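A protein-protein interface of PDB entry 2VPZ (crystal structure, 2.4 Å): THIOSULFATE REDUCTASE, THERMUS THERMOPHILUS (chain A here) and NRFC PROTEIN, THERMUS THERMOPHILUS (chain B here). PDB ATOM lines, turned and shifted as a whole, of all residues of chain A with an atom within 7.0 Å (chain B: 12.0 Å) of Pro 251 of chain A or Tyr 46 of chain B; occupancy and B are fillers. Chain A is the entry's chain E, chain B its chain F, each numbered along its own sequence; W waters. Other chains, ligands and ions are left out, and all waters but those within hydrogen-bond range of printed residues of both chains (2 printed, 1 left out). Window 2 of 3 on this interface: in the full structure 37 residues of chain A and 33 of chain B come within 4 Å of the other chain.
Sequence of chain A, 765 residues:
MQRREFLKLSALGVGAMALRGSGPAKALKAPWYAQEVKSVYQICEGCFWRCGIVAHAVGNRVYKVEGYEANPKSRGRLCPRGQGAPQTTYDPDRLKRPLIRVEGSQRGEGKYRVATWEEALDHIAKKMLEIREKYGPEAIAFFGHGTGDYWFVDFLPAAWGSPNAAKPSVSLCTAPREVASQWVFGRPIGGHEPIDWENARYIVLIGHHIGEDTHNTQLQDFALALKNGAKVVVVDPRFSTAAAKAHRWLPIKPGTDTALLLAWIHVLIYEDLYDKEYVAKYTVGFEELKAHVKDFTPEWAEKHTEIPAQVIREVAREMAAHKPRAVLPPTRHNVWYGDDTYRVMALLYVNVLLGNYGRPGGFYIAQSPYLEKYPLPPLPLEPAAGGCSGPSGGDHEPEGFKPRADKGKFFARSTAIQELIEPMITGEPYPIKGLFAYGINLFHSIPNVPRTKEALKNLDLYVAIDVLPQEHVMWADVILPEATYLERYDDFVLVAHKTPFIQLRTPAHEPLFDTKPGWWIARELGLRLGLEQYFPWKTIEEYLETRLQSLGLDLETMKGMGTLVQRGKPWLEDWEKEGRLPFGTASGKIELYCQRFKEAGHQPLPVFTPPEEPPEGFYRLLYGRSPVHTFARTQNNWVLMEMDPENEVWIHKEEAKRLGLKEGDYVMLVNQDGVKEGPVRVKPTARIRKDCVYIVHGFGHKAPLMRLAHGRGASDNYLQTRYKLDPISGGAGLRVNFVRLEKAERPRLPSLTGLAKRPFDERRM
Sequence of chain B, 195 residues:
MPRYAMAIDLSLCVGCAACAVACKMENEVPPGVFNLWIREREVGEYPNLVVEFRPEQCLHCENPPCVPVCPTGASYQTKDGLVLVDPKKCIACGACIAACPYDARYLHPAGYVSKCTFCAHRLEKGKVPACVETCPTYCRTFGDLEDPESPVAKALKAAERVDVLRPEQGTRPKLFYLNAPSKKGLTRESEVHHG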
ATOM      1  N   VAL A 234      33.718   1.373 -12.291  1.00  0.00           N
ATOM      2  CA  VAL A 234      32.902   0.590 -11.382  1.00  0.00           C
ATOM      3  C   VAL A 234      32.725  -0.806 -11.987  1.00  0.00           C
ATOM      4  O   VAL A 234      32.401  -0.913 -13.175  1.00  0.00           O
ATOM      5  CB  VAL A 234      31.536   1.361 -11.125  1.00  0.00           C
ATOM      6  CG1 VAL A 234      30.527   0.543 -10.277  1.00  0.00           C
ATOM      7  CG2 VAL A 234      31.854   2.671 -10.409  1.00  0.00           C
ATOM      8  N   VAL A 235      33.019  -1.857 -11.217  1.00  0.00           N
ATOM      9  CA  VAL A 235      32.876  -3.283 -11.625  1.00  0.00           C
ATOM     10  C   VAL A 235      31.700  -3.792 -10.754  1.00  0.00           C
ATOM     11  O   VAL A 235      31.796  -3.816  -9.526  1.00  0.00           O
ATOM     12  CB  VAL A 235      34.201  -4.115 -11.383  1.00  0.00           C
ATOM     13  CG1 VAL A 235      34.028  -5.543 -11.917  1.00  0.00           C
ATOM     14  CG2 VAL A 235      35.405  -3.453 -12.086  1.00  0.00           C
ATOM     15  N   ASP A 236      30.609  -4.219 -11.392  1.00  0.00           N
ATOM     16  CA  ASP A 236      29.375  -4.541 -10.661  1.00  0.00           C
ATOM     17  C   ASP A 236      28.290  -4.960 -11.697  1.00  0.00           C
ATOM     18  O   ASP A 236      28.162  -4.307 -12.744  1.00  0.00           O
ATOM     19  CB  ASP A 236      28.953  -3.208  -9.958  1.00  0.00           C
ATOM     20  CG  ASP A 236      27.821  -3.334  -8.883  1.00  0.00           C
ATOM     21  OD1 ASP A 236      26.954  -4.240  -8.969  1.00  0.00           O
ATOM     22  OD2 ASP A 236      27.784  -2.481  -7.950  1.00  0.00           O
ATOM     23  N   PRO A 237      27.512  -6.044 -11.430  1.00  0.00           N
ATOM     24  CA  PRO A 237      26.460  -6.467 -12.373  1.00  0.00           C
ATOM     25  C   PRO A 237      25.231  -5.524 -12.427  1.00  0.00           C
ATOM     26  O   PRO A 237      24.325  -5.696 -13.265  1.00  0.00           O
ATOM     27  CB  PRO A 237      26.073  -7.868 -11.886  1.00  0.00           C
ATOM     28  CG  PRO A 237      26.422  -7.843 -10.395  1.00  0.00           C
ATOM     29  CD  PRO A 237      27.733  -7.063 -10.398  1.00  0.00           C
ATOM     30  N   ARG A 238      25.197  -4.542 -11.529  1.00  0.00           N
ATOM     31  CA  ARG A 238      24.073  -3.587 -11.422  1.00  0.00           C
ATOM     32  C   ARG A 238      24.532  -2.152 -11.770  1.00  0.00           C
ATOM     33  O   ARG A 238      25.639  -1.764 -11.349  1.00  0.00           O
ATOM     34  CB  ARG A 238      23.529  -3.629  -9.979  1.00  0.00           C
ATOM     35  CG  ARG A 238      22.278  -2.764  -9.709  1.00  0.00           C
ATOM     36  CD  ARG A 238      21.859  -2.770  -8.230  1.00  0.00           C
ATOM     37  NE  ARG A 238      22.851  -2.213  -7.310  1.00  0.00           N
ATOM     38  CZ  ARG A 238      22.805  -0.990  -6.786  1.00  0.00           C
ATOM     39  NH1 ARG A 238      21.800  -0.172  -7.104  1.00  0.00           N
ATOM     40  NH2 ARG A 238      23.734  -0.596  -5.910  1.00  0.00           N
ATOM     41  N   PHE A 239      23.781  -1.372 -12.543  1.00  0.00           N
ATOM     42  CA  PHE A 239      24.202   0.051 -12.790  1.00  0.00           C
ATOM     43  C   PHE A 239      23.791   0.781 -11.551  1.00  0.00           C
ATOM     44  O   PHE A 239      22.727   1.241 -11.397  1.00  0.00           O
ATOM     45  CB  PHE A 239      23.412   0.826 -13.875  1.00  0.00           C
ATOM     46  CG  PHE A 239      24.170   2.047 -14.460  1.00  0.00           C
ATOM     47  CD1 PHE A 239      25.401   1.843 -15.125  1.00  0.00           C
ATOM     48  CD2 PHE A 239      23.684   3.361 -14.346  1.00  0.00           C
ATOM     49  CE1 PHE A 239      26.146   2.944 -15.674  1.00  0.00           C
ATOM     50  CE2 PHE A 239      24.411   4.463 -14.899  1.00  0.00           C
ATOM     51  CZ  PHE A 239      25.639   4.253 -15.556  1.00  0.00           C
ATOM     52  N   TRP A 249      31.927   1.459 -16.861  1.00  0.00           N
ATOM     53  CA  TRP A 249      31.127   0.552 -16.045  1.00  0.00           C
ATOM     54  C   TRP A 249      31.398  -0.851 -16.611  1.00  0.00           C
ATOM     55  O   TRP A 249      31.164  -1.064 -17.794  1.00  0.00           O
ATOM     56  CB  TRP A 249      29.606   0.832 -16.134  1.00  0.00           C
ATOM     57  CG  TRP A 249      28.731  -0.251 -15.451  1.00  0.00           C
ATOM     58  CD1 TRP A 249      28.974  -0.867 -14.248  1.00  0.00           C
ATOM     59  CD2 TRP A 249      27.481  -0.810 -15.932  1.00  0.00           C
ATOM     60  NE1 TRP A 249      27.970  -1.764 -13.965  1.00  0.00           N
ATOM     61  CE2 TRP A 249      27.049  -1.758 -14.977  1.00  0.00           C
ATOM     62  CE3 TRP A 249      26.702  -0.612 -17.085  1.00  0.00           C
ATOM     63  CZ2 TRP A 249      25.846  -2.499 -15.124  1.00  0.00           C
ATOM     64  CZ3 TRP A 249      25.500  -1.347 -17.242  1.00  0.00           C
ATOM     65  CH2 TRP A 249      25.098  -2.287 -16.262  1.00  0.00           C
ATOM     66  N   LEU A 250      31.915  -1.800 -15.830  1.00  0.00           N
ATOM     67  CA  LEU A 250      32.110  -3.158 -16.373  1.00  0.00           C
ATOM     68  C   LEU A 250      30.959  -4.026 -15.804  1.00  0.00           C
ATOM     69  O   LEU A 250      30.973  -4.382 -14.622  1.00  0.00           O
ATOM     70  CB  LEU A 250      33.500  -3.744 -16.016  1.00  0.00           C
ATOM     71  CG  LEU A 250      34.819  -2.934 -16.028  1.00  0.00           C
ATOM     72  CD1 LEU A 250      35.949  -3.881 -16.415  1.00  0.00           C
ATOM     73  CD2 LEU A 250      34.818  -1.742 -17.002  1.00  0.00           C
ATOM     74  N   PRO A 251      29.939  -4.374 -16.628  1.00  0.00           N
ATOM     75  CA  PRO A 251      28.886  -5.190 -16.002  1.00  0.00           C
ATOM     76  C   PRO A 251      29.235  -6.677 -15.854  1.00  0.00           C
ATOM     77  O   PRO A 251      28.692  -7.531 -16.562  1.00  0.00           O
ATOM     78  CB  PRO A 251      27.674  -4.947 -16.888  1.00  0.00           C
ATOM     79  CG  PRO A 251      28.285  -4.747 -18.284  1.00  0.00           C
ATOM     80  CD  PRO A 251      29.660  -4.104 -18.050  1.00  0.00           C
ATOM     81  N   ILE A 252      30.113  -6.967 -14.900  1.00  0.00           N
ATOM     82  CA  ILE A 252      30.633  -8.308 -14.659  1.00  0.00           C
ATOM     83  C   ILE A 252      29.607  -9.387 -14.298  1.00  0.00           C
ATOM     84  O   ILE A 252      28.563  -9.104 -13.707  1.00  0.00           O
ATOM     85  CB  ILE A 252      31.775  -8.234 -13.567  1.00  0.00           C
ATOM     86  CG1 ILE A 252      32.736  -9.416 -13.705  1.00  0.00           C
ATOM     87  CG2 ILE A 252      31.144  -8.092 -12.182  1.00  0.00           C
ATOM     88  CD1 ILE A 252      33.998  -9.322 -12.808  1.00  0.00           C
ATOM     89  N   LYS A 253      29.887 -10.622 -14.699  1.00  0.00           N
ATOM     90  CA  LYS A 253      29.017 -11.729 -14.362  1.00  0.00           C
ATOM     91  C   LYS A 253      29.241 -12.027 -12.871  1.00  0.00           C
ATOM     92  O   LYS A 253      30.387 -12.166 -12.420  1.00  0.00           O
ATOM     93  CB  LYS A 253      29.332 -12.945 -15.211  1.00  0.00           C
ATOM     94  CG  LYS A 253      28.357 -14.056 -14.996  1.00  0.00           C
ATOM     95  CD  LYS A 253      28.773 -15.208 -15.837  1.00  0.00           C
ATOM     96  CE  LYS A 253      28.446 -16.495 -15.162  1.00  0.00           C
ATOM     97  NZ  LYS A 253      28.769 -17.570 -16.108  1.00  0.00           N
ATOM     98  N   PRO A 254      28.152 -12.130 -12.081  1.00  0.00           N
ATOM     99  CA  PRO A 254      28.354 -12.399 -10.650  1.00  0.00           C
ATOM    100  C   PRO A 254      29.232 -13.618 -10.226  1.00  0.00           C
ATOM    101  O   PRO A 254      29.139 -14.700 -10.829  1.00  0.00           O
ATOM    102  CB  PRO A 254      26.936 -12.467 -10.062  1.00  0.00           C
ATOM    103  CG  PRO A 254      25.963 -12.226 -11.205  1.00  0.00           C
ATOM    104  CD  PRO A 254      26.742 -11.938 -12.457  1.00  0.00           C
ATOM    105  N   THR A 305      34.135 -14.100 -17.228  1.00  0.00           N
ATOM    106  CA  THR A 305      33.788 -12.767 -16.823  1.00  0.00           C
ATOM    107  C   THR A 305      32.742 -12.035 -17.686  1.00  0.00           C
ATOM    108  O   THR A 305      31.861 -11.314 -17.183  1.00  0.00           O
ATOM    109  CB  THR A 305      35.197 -12.042 -16.752  1.00  0.00           C
ATOM    110  OG1 THR A 305      35.550 -11.722 -15.418  1.00  0.00           O
ATOM    111  CG2 THR A 305      35.268 -10.874 -17.656  1.00  0.00           C
ATOM    112  N   GLU A 306      32.852 -12.283 -18.979  1.00  0.00           N
ATOM    113  CA  GLU A 306      32.065 -11.694 -20.036  1.00  0.00           C
ATOM    114  C   GLU A 306      32.511 -10.229 -20.293  1.00  0.00           C
ATOM    115  O   GLU A 306      31.856  -9.501 -21.023  1.00  0.00           O
ATOM    116  CB  GLU A 306      30.569 -11.801 -19.769  1.00  0.00           C
ATOM    117  CG  GLU A 306      30.088 -13.202 -19.398  1.00  0.00           C
ATOM    118  CD  GLU A 306      28.570 -13.336 -19.420  1.00  0.00           C
ATOM    119  OE1 GLU A 306      27.893 -12.286 -19.458  1.00  0.00           O
ATOM    120  OE2 GLU A 306      28.068 -14.486 -19.398  1.00  0.00           O
ATOM    121  N   ILE A 307      33.613  -9.793 -19.676  1.00  0.00           N
ATOM    122  CA  ILE A 307      34.178  -8.451 -19.925  1.00  0.00           C
ATOM    123  C   ILE A 307      35.152  -8.686 -21.133  1.00  0.00           C
ATOM    124  O   ILE A 307      36.015  -9.584 -21.072  1.00  0.00           O
ATOM    125  CB  ILE A 307      34.886  -7.858 -18.633  1.00  0.00           C
ATOM    126  CG1 ILE A 307      33.875  -7.818 -17.487  1.00  0.00           C
ATOM    127  CG2 ILE A 307      35.473  -6.431 -18.918  1.00  0.00           C
ATOM    128  CD1 ILE A 307      32.600  -7.006 -17.789  1.00  0.00           C
ATOM    129  N   PRO A 308      35.001  -7.913 -22.246  1.00  0.00           N
ATOM    130  CA  PRO A 308      35.891  -8.132 -23.398  1.00  0.00           C
ATOM    131  C   PRO A 308      37.407  -7.962 -23.102  1.00  0.00           C
ATOM    132  O   PRO A 308      37.807  -7.020 -22.405  1.00  0.00           O
ATOM    133  CB  PRO A 308      35.335  -7.185 -24.495  1.00  0.00           C
ATOM    134  CG  PRO A 308      33.980  -6.700 -23.954  1.00  0.00           C
ATOM    135  CD  PRO A 308      34.174  -6.715 -22.440  1.00  0.00           C
ATOM    136  N   VAL A 311      38.944  -4.553 -23.128  1.00  0.00           N
ATOM    137  CA  VAL A 311      38.607  -3.613 -22.029  1.00  0.00           C
ATOM    138  C   VAL A 311      39.390  -3.969 -20.761  1.00  0.00           C
ATOM    139  O   VAL A 311      39.777  -3.086 -19.996  1.00  0.00           O
ATOM    140  CB  VAL A 311      37.041  -3.536 -21.741  1.00  0.00           C
ATOM    141  CG1 VAL A 311      36.731  -2.992 -20.337  1.00  0.00           C
ATOM    142  CG2 VAL A 311      36.382  -2.616 -22.779  1.00  0.00           C
ATOM    143  N   HIS A 652      15.423  -6.817 -15.005  1.00  0.00           N
ATOM    144  CA  HIS A 652      15.585  -6.189 -16.293  1.00  0.00           C
ATOM    145  C   HIS A 652      14.232  -6.042 -16.995  1.00  0.00           C
ATOM    146  O   HIS A 652      13.366  -6.914 -16.891  1.00  0.00           O
ATOM    147  CB  HIS A 652      16.564  -7.007 -17.170  1.00  0.00           C
ATOM    148  CG  HIS A 652      17.082  -6.281 -18.362  1.00  0.00           C
ATOM    149  ND1 HIS A 652      16.441  -6.292 -19.570  1.00  0.00           N
ATOM    150  CD2 HIS A 652      18.171  -5.515 -18.526  1.00  0.00           C
ATOM    151  CE1 HIS A 652      17.115  -5.556 -20.425  1.00  0.00           C
ATOM    152  NE2 HIS A 652      18.172  -5.072 -19.813  1.00  0.00           N
ATOM    153  N   ALA A 686      15.838  -1.000 -16.209  1.00  0.00           N
ATOM    154  CA  ALA A 686      17.126  -1.431 -16.923  1.00  0.00           C
ATOM    155  C   ALA A 686      18.670  -1.380 -16.503  1.00  0.00           C
ATOM    156  O   ALA A 686      19.605  -1.549 -17.324  1.00  0.00           O
ATOM    157  CB  ALA A 686      17.041  -0.708 -18.261  1.00  0.00           C
ATOM    158  N   ARG A 689      21.807  -6.841 -14.918  1.00  0.00           N
ATOM    159  CA  ARG A 689      21.870  -7.976 -15.850  1.00  0.00           C
ATOM    160  C   ARG A 689      20.566  -8.821 -15.711  1.00  0.00           C
ATOM    161  O   ARG A 689      19.805  -8.653 -14.750  1.00  0.00           O
ATOM    162  CB  ARG A 689      23.108  -8.844 -15.603  1.00  0.00           C
ATOM    163  CG  ARG A 689      24.438  -8.172 -15.975  1.00  0.00           C
ATOM    164  CD  ARG A 689      25.577  -8.854 -15.244  1.00  0.00           C
ATOM    165  NE  ARG A 689      25.564 -10.277 -15.541  1.00  0.00           N
ATOM    166  CZ  ARG A 689      26.198 -10.844 -16.556  1.00  0.00           C
ATOM    167  NH1 ARG A 689      26.922 -10.104 -17.372  1.00  0.00           N
ATOM    168  NH2 ARG A 689      26.078 -12.149 -16.794  1.00  0.00           N
ATOM    169  N   GLU B  42      16.209   7.309 -14.856  1.00  0.00           N
ATOM    170  CA  GLU B  42      17.188   6.671 -15.758  1.00  0.00           C
ATOM    171  C   GLU B  42      16.811   7.013 -17.239  1.00  0.00           C
ATOM    172  O   GLU B  42      15.623   7.189 -17.546  1.00  0.00           O
ATOM    173  CB  GLU B  42      17.266   5.138 -15.529  1.00  0.00           C
ATOM    174  CG  GLU B  42      16.082   4.294 -16.022  1.00  0.00           C
ATOM    175  CD  GLU B  42      16.164   2.808 -15.614  1.00  0.00           C
ATOM    176  OE1 GLU B  42      16.324   1.945 -16.514  1.00  0.00           O
ATOM    177  OE2 GLU B  42      16.074   2.512 -14.397  1.00  0.00           O
ATOM    178  N   VAL B  43      17.811   7.168 -18.115  1.00  0.00           N
ATOM    179  CA  VAL B  43      17.667   7.489 -19.559  1.00  0.00           C
ATOM    180  C   VAL B  43      18.491   6.340 -20.050  1.00  0.00           C
ATOM    181  O   VAL B  43      19.690   6.247 -19.772  1.00  0.00           O
ATOM    182  CB  VAL B  43      18.247   8.850 -19.893  1.00  0.00           C
ATOM    183  CG1 VAL B  43      17.917   9.207 -21.322  1.00  0.00           C
ATOM    184  CG2 VAL B  43      17.642   9.886 -18.975  1.00  0.00           C
ATOM    185  N   GLY B  44      17.852   5.506 -20.847  1.00  0.00           N
ATOM    186  CA  GLY B  44      18.465   4.222 -21.041  1.00  0.00           C
ATOM    187  C   GLY B  44      19.147   3.479 -22.123  1.00  0.00           C
ATOM    188  O   GLY B  44      19.430   4.052 -23.151  1.00  0.00           O
ATOM    189  N   GLU B  45      19.425   2.198 -21.848  1.00  0.00           N
ATOM    190  CA  GLU B  45      20.105   1.238 -22.743  1.00  0.00           C
ATOM    191  C   GLU B  45      21.640   1.157 -22.535  1.00  0.00           C
ATOM    192  O   GLU B  45      22.366   2.106 -22.852  1.00  0.00           O
ATOM    193  CB  GLU B  45      19.763   1.552 -24.197  1.00  0.00           C
ATOM    194  CG  GLU B  45      18.293   1.345 -24.586  1.00  0.00           C
ATOM    195  CD  GLU B  45      17.970  -0.103 -24.970  1.00  0.00           C
ATOM    196  OE1 GLU B  45      18.000  -0.982 -24.073  1.00  0.00           O
ATOM    197  OE2 GLU B  45      17.701  -0.339 -26.175  1.00  0.00           O
ATOM    198  N   TYR B  46      22.107  -0.002 -22.050  1.00  0.00           N
ATOM    199  CA  TYR B  46      23.519  -0.332 -21.684  1.00  0.00           C
ATOM    200  C   TYR B  46      24.780   0.527 -21.948  1.00  0.00           C
ATOM    201  O   TYR B  46      25.256   1.184 -20.995  1.00  0.00           O
ATOM    202  CB  TYR B  46      23.885  -1.796 -22.060  1.00  0.00           C
ATOM    203  CG  TYR B  46      25.390  -2.152 -21.948  1.00  0.00           C
ATOM    204  CD1 TYR B  46      26.148  -1.750 -20.841  1.00  0.00           C
ATOM    205  CD2 TYR B  46      26.047  -2.883 -22.957  1.00  0.00           C
ATOM    206  CE1 TYR B  46      27.519  -2.055 -20.732  1.00  0.00           C
ATOM    207  CE2 TYR B  46      27.434  -3.201 -22.862  1.00  0.00           C
ATOM    208  CZ  TYR B  46      28.167  -2.781 -21.747  1.00  0.00           C
ATOM    209  OH  TYR B  46      29.520  -3.073 -21.655  1.00  0.00           O
ATOM    210  N   PRO B  47      25.363   0.510 -23.190  1.00  0.00           N
ATOM    211  CA  PRO B  47      26.565   1.308 -23.466  1.00  0.00           C
ATOM    212  C   PRO B  47      26.357   2.788 -23.223  1.00  0.00           C
ATOM    213  O   PRO B  47      27.317   3.562 -23.087  1.00  0.00           O
ATOM    214  CB  PRO B  47      26.896   1.001 -24.946  1.00  0.00           C
ATOM    215  CG  PRO B  47      25.593   0.609 -25.553  1.00  0.00           C
ATOM    216  CD  PRO B  47      24.826  -0.066 -24.432  1.00  0.00           C
ATOM    217  N   ASN B  48      25.084   3.134 -23.108  1.00  0.00           N
ATOM    218  CA  ASN B  48      24.620   4.502 -22.973  1.00  0.00           C
ATOM    219  C   ASN B  48      23.550   4.762 -21.875  1.00  0.00           C
ATOM    220  O   ASN B  48      22.534   5.411 -22.139  1.00  0.00           O
ATOM    221  CB  ASN B  48      24.092   4.955 -24.368  1.00  0.00           C
ATOM    222  CG  ASN B  48      25.147   4.798 -25.526  1.00  0.00           C
ATOM    223  OD1 ASN B  48      26.218   5.418 -25.499  1.00  0.00           O
ATOM    224  ND2 ASN B  48      24.818   3.979 -26.537  1.00  0.00           N
ATOM    225  N   LEU B  49      23.784   4.256 -20.664  1.00  0.00           N
ATOM    226  CA  LEU B  49      22.887   4.434 -19.513  1.00  0.00           C
ATOM    227  C   LEU B  49      23.273   5.759 -18.823  1.00  0.00           C
ATOM    228  O   LEU B  49      24.465   6.026 -18.672  1.00  0.00           O
ATOM    229  CB  LEU B  49      23.088   3.292 -18.499  1.00  0.00           C
ATOM    230  CG  LEU B  49      21.969   2.510 -17.827  1.00  0.00           C
ATOM    231  CD1 LEU B  49      20.694   2.703 -18.608  1.00  0.00           C
ATOM    232  CD2 LEU B  49      22.360   1.021 -17.747  1.00  0.00           C
ATOM    233  N   VAL B  50      22.286   6.570 -18.429  1.00  0.00           N
ATOM    234  CA  VAL B  50      22.477   7.837 -17.688  1.00  0.00           C
ATOM    235  C   VAL B  50      21.419   7.946 -16.529  1.00  0.00           C
ATOM    236  O   VAL B  50      20.247   7.617 -16.746  1.00  0.00           O
ATOM    237  CB  VAL B  50      22.410   9.095 -18.666  1.00  0.00           C
ATOM    238  CG1 VAL B  50      22.273  10.429 -17.877  1.00  0.00           C
ATOM    239  CG2 VAL B  50      23.683   9.136 -19.534  1.00  0.00           C
ATOM    240  N   VAL B  51      21.832   8.304 -15.300  1.00  0.00           N
ATOM    241  CA  VAL B  51      20.898   8.499 -14.150  1.00  0.00           C
ATOM    242  C   VAL B  51      21.049   9.949 -13.647  1.00  0.00           C
ATOM    243  O   VAL B  51      22.161  10.431 -13.392  1.00  0.00           O
ATOM    244  CB  VAL B  51      21.100   7.516 -12.867  1.00  0.00           C
ATOM    245  CG1 VAL B  51      19.903   7.678 -11.854  1.00  0.00           C
ATOM    246  CG2 VAL B  51      21.181   6.055 -13.290  1.00  0.00           C
HETATM  247  O   HOH W   1      18.043  -2.318 -21.652  1.00  0.00           O
HETATM  248  O   HOH W   2      29.850  -0.682 -20.151  1.00  0.00           O
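The backbone NH of Ala 686 of chain A sits at hydrogen-bond distance from the side-chain carboxylate of Glu 42 of chain B (3.0 Å).
NE1 of Trp 249 of chain A sits at hydrogen-bond distance from O of Asp 236 of chain A (2.8 Å). NH1 of Arg 689 of chain A lies within hydrogen-bond range of O of Pro 251 of chain A, at 3.2 Å.
Among the printed residues, pairs that only touch across the chains: Trp 249 of chain A with Tyr 46 of chain B (3.7 Å), Pro 251 of chain A with Tyr 46 of chain B (3.7 Å), Phe 239 of chain A with Leu 49 of chain B (3.8 Å), Ala 686 of chain A with Leu 49 of chain B (3.8 Å), Phe 239 of chain A with Val 51 of chain B (3.8 Å) and Trp 249 of chain A with Leu 49 of chain B (3.97 Å).
No residue of chain B comes within 4 Å of Val 235 of chain A. Pro 237 of chain A touches none of the printed residues of chain B. Of the printed residues of chain B, Phe 239 of chain A touches Leu 49 (3.8 Å) and Val 51 (3.8 Å). Of chain B, only Tyr 46 (3.7 Å) and Leu 49 (3.97 Å) come within 4 Å of Trp 249 of chain A. Of chain B, only Tyr 46 comes within 4 Å of Pro 251 of chain A. Of chain A, only Trp 249 and Pro 251 come within 4 Å of Tyr 46 of chain B. Of the printed residues of chain A, Val 51 of chain B touches Phe 239. The nearest residue of chain A that does not touch Tyr 46 of chain B is Ala 686 of chain A (5.6 Å). The nearest printed residue of chain A that does not touch Glu 42 of chain B is Phe 239 of chain A (6.8 Å).
Printed residues of chain B that touch a printed residue of chain A: Glu 42, Tyr 46, Leu 49 and Val 51. Hydrophobic or aromatic side chains of chain B that line the printed part of chain A: Tyr 46, Leu 49 and Val 51. Along chain B the printed residues that touch a printed residue of chain A span positions 42 to 51. Printed residues of chain A that touch a printed residue of chain B: Phe 239, Trp 249, Pro 251 and Ala 686. Hydrophobic or aromatic side chains of chain A that line the printed part of chain B: Phe 239, Trp 249, Pro 251 and Ala 686. Among the printed residues, 7 pairs touch across the chains. Among the printed residues, no Asp or Glu carboxylate lies within 4 Å of a Lys or Arg side-chain nitrogen of the other chain.
Water W2 lies within hydrogen-bond range of the backbone carbonyl oxygen (O) of Trp 249 of chain A and the side-chain hydroxyl (OH) of Tyr 46 of chain B. Water W1 lies within hydrogen-bond range of the side-chain carboxylate (OE1) of Glu 45 of chain B (2.8 Å) and a ring nitrogen (NE2) of His 652 of chain A (3.3 Å).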
